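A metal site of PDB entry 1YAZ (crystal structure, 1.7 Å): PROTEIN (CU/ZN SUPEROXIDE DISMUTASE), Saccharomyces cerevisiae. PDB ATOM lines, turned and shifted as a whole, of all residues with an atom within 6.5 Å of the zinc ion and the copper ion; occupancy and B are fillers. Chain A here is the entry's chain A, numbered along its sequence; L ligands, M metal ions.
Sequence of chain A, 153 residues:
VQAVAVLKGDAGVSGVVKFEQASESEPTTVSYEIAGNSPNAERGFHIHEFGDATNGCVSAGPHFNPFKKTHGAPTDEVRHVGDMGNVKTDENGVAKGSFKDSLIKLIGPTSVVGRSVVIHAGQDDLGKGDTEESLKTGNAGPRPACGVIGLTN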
ATOM      1  N   GLY A  44       9.473  26.212 -25.605  1.00  0.00           N
ATOM      2  CA  GLY A  44       8.686  26.112 -24.374  1.00  0.00           C
ATOM      3  C   GLY A  44       9.184  25.009 -23.467  1.00  0.00           C
ATOM      4  O   GLY A  44       9.483  23.909 -23.916  1.00  0.00           O
ATOM      5  N   PHE A  45       9.259  25.308 -22.176  1.00  0.00           N
ATOM      6  CA  PHE A  45       9.866  24.305 -21.227  1.00  0.00           C
ATOM      7  C   PHE A  45       8.963  24.303 -19.993  1.00  0.00           C
ATOM      8  O   PHE A  45       8.864  25.333 -19.304  1.00  0.00           O
ATOM      9  CB  PHE A  45      11.245  24.936 -20.886  1.00  0.00           C
ATOM     10  CG  PHE A  45      12.114  24.091 -19.991  1.00  0.00           C
ATOM     11  CD1 PHE A  45      12.255  22.734 -20.187  1.00  0.00           C
ATOM     12  CD2 PHE A  45      12.748  24.702 -18.906  1.00  0.00           C
ATOM     13  CE1 PHE A  45      13.068  21.980 -19.360  1.00  0.00           C
ATOM     14  CE2 PHE A  45      13.636  23.962 -18.133  1.00  0.00           C
ATOM     15  CZ  PHE A  45      13.776  22.609 -18.346  1.00  0.00           C
ATOM     16  N   HIS A  46       8.227  23.212 -19.788  1.00  0.00           N
ATOM     17  CA  HIS A  46       7.198  23.246 -18.734  1.00  0.00           C
ATOM     18  C   HIS A  46       7.196  21.977 -17.874  1.00  0.00           C
ATOM     19  O   HIS A  46       7.660  20.921 -18.235  1.00  0.00           O
ATOM     20  CB  HIS A  46       5.814  23.244 -19.465  1.00  0.00           C
ATOM     21  CG  HIS A  46       5.688  24.359 -20.455  1.00  0.00           C
ATOM     22  ND1 HIS A  46       5.059  24.184 -21.667  1.00  0.00           N
ATOM     23  CD2 HIS A  46       6.103  25.648 -20.409  1.00  0.00           C
ATOM     24  CE1 HIS A  46       5.078  25.322 -22.330  1.00  0.00           C
ATOM     25  NE2 HIS A  46       5.704  26.245 -21.590  1.00  0.00           N
ATOM     26  N   ILE A  47       6.535  22.125 -16.701  1.00  0.00           N
ATOM     27  CA  ILE A  47       6.304  20.943 -15.858  1.00  0.00           C
ATOM     28  C   ILE A  47       4.808  20.630 -15.983  1.00  0.00           C
ATOM     29  O   ILE A  47       3.977  21.526 -15.869  1.00  0.00           O
ATOM     30  CB  ILE A  47       6.597  21.284 -14.359  1.00  0.00           C
ATOM     31  CG1 ILE A  47       8.118  21.519 -14.221  1.00  0.00           C
ATOM     32  CG2 ILE A  47       6.182  20.016 -13.540  1.00  0.00           C
ATOM     33  CD1 ILE A  47       8.662  21.761 -12.890  1.00  0.00           C
ATOM     34  N   HIS A  48       4.555  19.406 -16.408  1.00  0.00           N
ATOM     35  CA  HIS A  48       3.201  18.927 -16.673  1.00  0.00           C
ATOM     36  C   HIS A  48       2.704  18.086 -15.513  1.00  0.00           C
ATOM     37  O   HIS A  48       3.512  17.615 -14.702  1.00  0.00           O
ATOM     38  CB  HIS A  48       3.169  18.131 -17.969  1.00  0.00           C
ATOM     39  CG  HIS A  48       3.306  19.025 -19.181  1.00  0.00           C
ATOM     40  ND1 HIS A  48       2.504  18.856 -20.271  1.00  0.00           N
ATOM     41  CD2 HIS A  48       4.166  20.012 -19.455  1.00  0.00           C
ATOM     42  CE1 HIS A  48       2.869  19.746 -21.208  1.00  0.00           C
ATOM     43  NE2 HIS A  48       3.853  20.473 -20.756  1.00  0.00           N
ATOM     44  N   PRO A  62      -1.704  18.115 -18.963  1.00  0.00           N
ATOM     45  CA  PRO A  62      -1.522  19.560 -19.151  1.00  0.00           C
ATOM     46  C   PRO A  62      -0.502  20.122 -18.167  1.00  0.00           C
ATOM     47  O   PRO A  62       0.136  19.399 -17.407  1.00  0.00           O
ATOM     48  CB  PRO A  62      -2.941  20.089 -18.716  1.00  0.00           C
ATOM     49  CG  PRO A  62      -3.259  19.192 -17.571  1.00  0.00           C
ATOM     50  CD  PRO A  62      -2.790  17.808 -18.014  1.00  0.00           C
ATOM     51  N   HIS A  63      -0.327  21.441 -18.185  1.00  0.00           N
ATOM     52  CA  HIS A  63       0.685  22.005 -17.242  1.00  0.00           C
ATOM     53  C   HIS A  63       0.197  21.841 -15.780  1.00  0.00           C
ATOM     54  O   HIS A  63      -0.998  21.894 -15.468  1.00  0.00           O
ATOM     55  CB  HIS A  63       0.762  23.526 -17.534  1.00  0.00           C
ATOM     56  CG  HIS A  63       1.474  23.769 -18.834  1.00  0.00           C
ATOM     57  ND1 HIS A  63       1.673  24.981 -19.398  1.00  0.00           N
ATOM     58  CD2 HIS A  63       2.067  22.854 -19.687  1.00  0.00           C
ATOM     59  CE1 HIS A  63       2.360  24.883 -20.521  1.00  0.00           C
ATOM     60  NE2 HIS A  63       2.575  23.583 -20.704  1.00  0.00           N
ATOM     61  N   PHE A  64       1.184  21.648 -14.913  1.00  0.00           N
ATOM     62  CA  PHE A  64       0.925  21.525 -13.473  1.00  0.00           C
ATOM     63  C   PHE A  64       0.372  22.865 -12.964  1.00  0.00           C
ATOM     64  O   PHE A  64       1.024  23.884 -13.114  1.00  0.00           O
ATOM     65  CB  PHE A  64       2.184  21.139 -12.746  1.00  0.00           C
ATOM     66  CG  PHE A  64       1.944  20.870 -11.242  1.00  0.00           C
ATOM     67  CD1 PHE A  64       0.848  20.177 -10.821  1.00  0.00           C
ATOM     68  CD2 PHE A  64       2.831  21.405 -10.327  1.00  0.00           C
ATOM     69  CE1 PHE A  64       0.620  20.010  -9.445  1.00  0.00           C
ATOM     70  CE2 PHE A  64       2.633  21.198  -8.954  1.00  0.00           C
ATOM     71  CZ  PHE A  64       1.512  20.521  -8.535  1.00  0.00           C
ATOM     72  N   THR A  70      -4.208  30.926 -15.264  1.00  0.00           N
ATOM     73  CA  THR A  70      -3.987  30.723 -16.712  1.00  0.00           C
ATOM     74  C   THR A  70      -2.481  30.705 -16.952  1.00  0.00           C
ATOM     75  O   THR A  70      -1.658  31.129 -16.149  1.00  0.00           O
ATOM     76  CB  THR A  70      -4.625  31.876 -17.512  1.00  0.00           C
ATOM     77  OG1 THR A  70      -4.288  33.122 -16.905  1.00  0.00           O
ATOM     78  CG2 THR A  70      -6.150  31.766 -17.496  1.00  0.00           C
ATOM     79  N   HIS A  71      -2.119  30.267 -18.147  1.00  0.00           N
ATOM     80  CA  HIS A  71      -0.698  30.168 -18.498  1.00  0.00           C
ATOM     81  C   HIS A  71      -0.030  31.516 -18.573  1.00  0.00           C
ATOM     82  O   HIS A  71      -0.616  32.517 -19.041  1.00  0.00           O
ATOM     83  CB  HIS A  71      -0.679  29.532 -19.937  1.00  0.00           C
ATOM     84  CG  HIS A  71       0.721  29.321 -20.427  1.00  0.00           C
ATOM     85  ND1 HIS A  71       1.497  28.277 -19.948  1.00  0.00           N
ATOM     86  CD2 HIS A  71       1.448  29.984 -21.351  1.00  0.00           C
ATOM     87  CE1 HIS A  71       2.680  28.328 -20.570  1.00  0.00           C
ATOM     88  NE2 HIS A  71       2.683  29.359 -21.412  1.00  0.00           N
ATOM     89  N   GLY A  72       1.258  31.571 -18.222  1.00  0.00           N
ATOM     90  CA  GLY A  72       1.993  32.811 -18.322  1.00  0.00           C
ATOM     91  C   GLY A  72       3.493  32.634 -18.339  1.00  0.00           C
ATOM     92  O   GLY A  72       4.011  31.513 -18.474  1.00  0.00           O
ATOM     93  N   ARG A  79       0.359  32.727 -13.494  1.00  0.00           N
ATOM     94  CA  ARG A  79       1.010  31.682 -14.316  1.00  0.00           C
ATOM     95  C   ARG A  79       0.644  30.312 -13.697  1.00  0.00           C
ATOM     96  O   ARG A  79       0.174  30.275 -12.559  1.00  0.00           O
ATOM     97  CB  ARG A  79       2.551  31.827 -14.215  1.00  0.00           C
ATOM     98  CG  ARG A  79       3.104  31.862 -12.801  1.00  0.00           C
ATOM     99  CD  ARG A  79       4.641  31.851 -12.794  1.00  0.00           C
ATOM    100  NE  ARG A  79       5.140  30.466 -12.685  1.00  0.00           N
ATOM    101  CZ  ARG A  79       6.330  30.145 -12.201  1.00  0.00           C
ATOM    102  NH1 ARG A  79       7.256  31.062 -11.944  1.00  0.00           N
ATOM    103  NH2 ARG A  79       6.615  28.854 -11.926  1.00  0.00           N
ATOM    104  N   HIS A  80       0.915  29.288 -14.435  1.00  0.00           N
ATOM    105  CA  HIS A  80       0.798  27.900 -13.880  1.00  0.00           C
ATOM    106  C   HIS A  80       2.047  27.696 -13.017  1.00  0.00           C
ATOM    107  O   HIS A  80       3.122  28.228 -13.339  1.00  0.00           O
ATOM    108  CB  HIS A  80       0.861  26.940 -15.066  1.00  0.00           C
ATOM    109  CG  HIS A  80      -0.366  27.037 -15.928  1.00  0.00           C
ATOM    110  ND1 HIS A  80      -0.365  26.790 -17.266  1.00  0.00           N
ATOM    111  CD2 HIS A  80      -1.642  27.335 -15.604  1.00  0.00           C
ATOM    112  CE1 HIS A  80      -1.591  26.869 -17.771  1.00  0.00           C
ATOM    113  NE2 HIS A  80      -2.400  27.223 -16.762  1.00  0.00           N
ATOM    114  N   GLY A  82       3.724  25.135 -13.244  1.00  0.00           N
ATOM    115  CA  GLY A  82       4.666  24.480 -14.166  1.00  0.00           C
ATOM    116  C   GLY A  82       5.278  25.361 -15.218  1.00  0.00           C
ATOM    117  O   GLY A  82       6.069  24.900 -16.058  1.00  0.00           O
ATOM    118  N   ASP A  83       4.971  26.664 -15.307  1.00  0.00           N
ATOM    119  CA  ASP A  83       5.448  27.430 -16.474  1.00  0.00           C
ATOM    120  C   ASP A  83       6.874  27.902 -16.308  1.00  0.00           C
ATOM    121  O   ASP A  83       7.106  28.873 -15.567  1.00  0.00           O
ATOM    122  CB  ASP A  83       4.539  28.740 -16.546  1.00  0.00           C
ATOM    123  CG  ASP A  83       3.163  28.346 -17.082  1.00  0.00           C
ATOM    124  OD1 ASP A  83       3.045  27.226 -17.618  1.00  0.00           O
ATOM    125  OD2 ASP A  83       2.206  29.154 -17.001  1.00  0.00           O
ATOM    126  N   VAL A 118       8.609  18.665 -19.775  1.00  0.00           N
ATOM    127  CA  VAL A 118       8.388  18.564 -21.226  1.00  0.00           C
ATOM    128  C   VAL A 118       9.143  19.711 -21.910  1.00  0.00           C
ATOM    129  O   VAL A 118       9.035  20.831 -21.462  1.00  0.00           O
ATOM    130  CB  VAL A 118       6.880  18.725 -21.535  1.00  0.00           C
ATOM    131  CG1 VAL A 118       6.691  18.968 -23.032  1.00  0.00           C
ATOM    132  CG2 VAL A 118       6.165  17.411 -21.138  1.00  0.00           C
ATOM    133  N   HIS A 120       9.192  21.624 -25.529  1.00  0.00           N
ATOM    134  CA  HIS A 120       8.282  21.613 -26.711  1.00  0.00           C
ATOM    135  C   HIS A 120       9.091  21.910 -27.988  1.00  0.00           C
ATOM    136  O   HIS A 120      10.253  22.294 -27.937  1.00  0.00           O
ATOM    137  CB  HIS A 120       7.287  22.805 -26.507  1.00  0.00           C
ATOM    138  CG  HIS A 120       6.156  22.437 -25.596  1.00  0.00           C
ATOM    139  ND1 HIS A 120       4.984  21.844 -26.030  1.00  0.00           N
ATOM    140  CD2 HIS A 120       5.994  22.693 -24.260  1.00  0.00           C
ATOM    141  CE1 HIS A 120       4.136  21.745 -24.989  1.00  0.00           C
ATOM    142  NE2 HIS A 120       4.765  22.210 -23.926  1.00  0.00           N
ATOM    143  N   ASP A 124       7.098  29.339 -26.679  1.00  0.00           N
ATOM    144  CA  ASP A 124       5.897  29.564 -25.738  1.00  0.00           C
ATOM    145  C   ASP A 124       5.548  31.056 -25.882  1.00  0.00           C
ATOM    146  O   ASP A 124       6.476  31.885 -25.772  1.00  0.00           O
ATOM    147  CB  ASP A 124       6.499  29.342 -24.325  1.00  0.00           C
ATOM    148  CG  ASP A 124       5.453  29.457 -23.231  1.00  0.00           C
ATOM    149  OD1 ASP A 124       4.477  30.206 -23.420  1.00  0.00           O
ATOM    150  OD2 ASP A 124       5.623  28.841 -22.153  1.00  0.00           O
ATOM    151  N   LEU A 135      -3.682  30.776 -23.498  1.00  0.00           N
ATOM    152  CA  LEU A 135      -3.923  30.803 -22.084  1.00  0.00           C
ATOM    153  C   LEU A 135      -3.826  29.434 -21.442  1.00  0.00           C
ATOM    154  O   LEU A 135      -3.848  29.380 -20.191  1.00  0.00           O
ATOM    155  CB  LEU A 135      -5.244  31.473 -21.733  1.00  0.00           C
ATOM    156  CG  LEU A 135      -5.336  32.966 -22.150  1.00  0.00           C
ATOM    157  CD1 LEU A 135      -6.733  33.489 -21.764  1.00  0.00           C
ATOM    158  CD2 LEU A 135      -4.281  33.753 -21.354  1.00  0.00           C
ATOM    159  N   LYS A 136      -3.655  28.402 -22.248  1.00  0.00           N
ATOM    160  CA  LYS A 136      -3.492  27.049 -21.778  1.00  0.00           C
ATOM    161  C   LYS A 136      -2.078  26.532 -21.886  1.00  0.00           C
ATOM    162  O   LYS A 136      -1.504  25.946 -20.966  1.00  0.00           O
ATOM    163  CB  LYS A 136      -4.442  26.086 -22.496  1.00  0.00           C
ATOM    164  CG  LYS A 136      -5.921  26.504 -22.350  1.00  0.00           C
ATOM    165  CD  LYS A 136      -5.967  28.023 -22.140  1.00  0.00           C
ATOM    166  CE  LYS A 136      -7.416  28.525 -22.221  1.00  0.00           C
ATOM    167  NZ  LYS A 136      -7.720  29.487 -21.110  1.00  0.00           N
ATOM    168  N   THR A 137      -1.478  26.634 -23.072  1.00  0.00           N
ATOM    169  CA  THR A 137      -0.148  26.001 -23.222  1.00  0.00           C
ATOM    170  C   THR A 137       0.881  26.993 -23.716  1.00  0.00           C
ATOM    171  O   THR A 137       2.037  26.629 -23.904  1.00  0.00           O
ATOM    172  CB  THR A 137      -0.244  24.909 -24.348  1.00  0.00           C
ATOM    173  OG1 THR A 137      -0.554  25.665 -25.568  1.00  0.00           O
ATOM    174  CG2 THR A 137      -1.446  24.033 -24.104  1.00  0.00           C
ATOM    175  N   GLY A 138       0.465  28.220 -24.067  1.00  0.00           N
ATOM    176  CA  GLY A 138       1.425  29.159 -24.644  1.00  0.00           C
ATOM    177  C   GLY A 138       1.579  28.891 -26.154  1.00  0.00           C
ATOM    178  O   GLY A 138       2.498  29.455 -26.749  1.00  0.00           O
ATOM    179  N   ALA A 140       2.782  26.347 -27.517  1.00  0.00           N
ATOM    180  CA  ALA A 140       4.150  25.871 -27.686  1.00  0.00           C
ATOM    181  C   ALA A 140       4.295  24.684 -28.596  1.00  0.00           C
ATOM    182  O   ALA A 140       5.441  24.261 -28.860  1.00  0.00           O
ATOM    183  CB  ALA A 140       4.814  25.627 -26.350  1.00  0.00           C
ATOM    184  N   GLY A 141       3.207  24.099 -29.103  1.00  0.00           N
ATOM    185  CA  GLY A 141       3.313  23.026 -30.066  1.00  0.00           C
ATOM    186  C   GLY A 141       3.631  21.664 -29.495  1.00  0.00           C
ATOM    187  O   GLY A 141       3.433  21.385 -28.307  1.00  0.00           O
ATOM    188  N   ARG A 143       5.480  17.960 -28.445  1.00  0.00           N
ATOM    189  CA  ARG A 143       6.315  17.652 -27.285  1.00  0.00           C
ATOM    190  C   ARG A 143       7.322  16.558 -27.724  1.00  0.00           C
ATOM    191  O   ARG A 143       7.044  15.387 -27.501  1.00  0.00           O
ATOM    192  CB  ARG A 143       5.351  16.920 -26.249  1.00  0.00           C
ATOM    193  CG  ARG A 143       4.204  17.827 -25.855  1.00  0.00           C
ATOM    194  CD  ARG A 143       3.256  17.085 -24.875  1.00  0.00           C
ATOM    195  NE  ARG A 143       2.122  17.993 -24.559  1.00  0.00           N
ATOM    196  CZ  ARG A 143       1.240  17.710 -23.611  1.00  0.00           C
ATOM    197  NH1 ARG A 143       1.401  16.618 -22.860  1.00  0.00           N
ATOM    198  NH2 ARG A 143       0.226  18.527 -23.384  1.00  0.00           N
HETATM  199  N1  LIG L   1       1.857  22.052 -23.136  1.00  0.00           N
HETATM  200  N2  LIG L   1       0.889  21.917 -22.437  1.00  0.00           N
HETATM  201  N3  LIG L   1      -0.086  21.408 -21.916  1.00  0.00           N
HETATM  202 ZN    ZN M   1       1.380  26.806 -18.538  1.00  0.00          ZN
HETATM  203 CU    CU M   2       3.654  22.794 -22.237  1.00  0.00          CU
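Merely in contact with the zinc ion: Lys 136.
Five residues have an atom within 4 Å of the zinc ion: His 63, His 71, His 80, Asp 83 and Lys 136.
The side-chain carboxylate (OD1) of Asp 83 binds the zinc ion.
ND1 of His 63 is bound to the zinc ion.
The zinc ion is bound by a ring nitrogen (ND1) of His 71, at 2.0 Å.
The zinc ion is bound by ND1 of His 80.
NE2 of His 63 sits close to NE2 of His 48, 3.4 Å away.
The backbone carbonyl oxygen (O) of Gly 141 lies within hydrogen-bond range of a ring nitrogen (ND1) of His 120 (2.8 Å).
A ring nitrogen (NE2) of His 71 is in hydrogen-bond range of the side-chain carboxylate of Asp 124 (2.8 Å).
The backbone NH (N) of Val 118 is in hydrogen-bond range of the backbone carbonyl oxygen (O) of His 46, 2.9 Å away.
The backbone NH of Gly 72 sits at hydrogen-bond distance from the side-chain carboxylate of Asp 83, at 2.9 Å.
A ring nitrogen (NE2) of His 46 is in hydrogen-bond range of the side-chain carboxylate of Asp 124, at 2.7 Å.
The backbone NH (N) of His 120 is in hydrogen-bond range of the backbone carbonyl oxygen (O) of Gly 44 (2.8 Å).
O of Leu 135 lies within hydrogen-bond range of N of His 71, at 2.8 Å.
The copper ion is bound by NE2 of His 63 (2.0 Å), ND1 of His 46 (2.1 Å), NE2 of His 120 (2.1 Å) and N1 of the ligand (2.1 Å).
Slightly farther from the copper ion lies a ring nitrogen (NE2) of His 48 (2.8 Å).
Four residues have an atom within 4 Å of the copper ion: His 46, His 48, His 63 and His 120.
The nearest printed residue that does not touch the copper ion is Thr 137 (4.5 Å).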
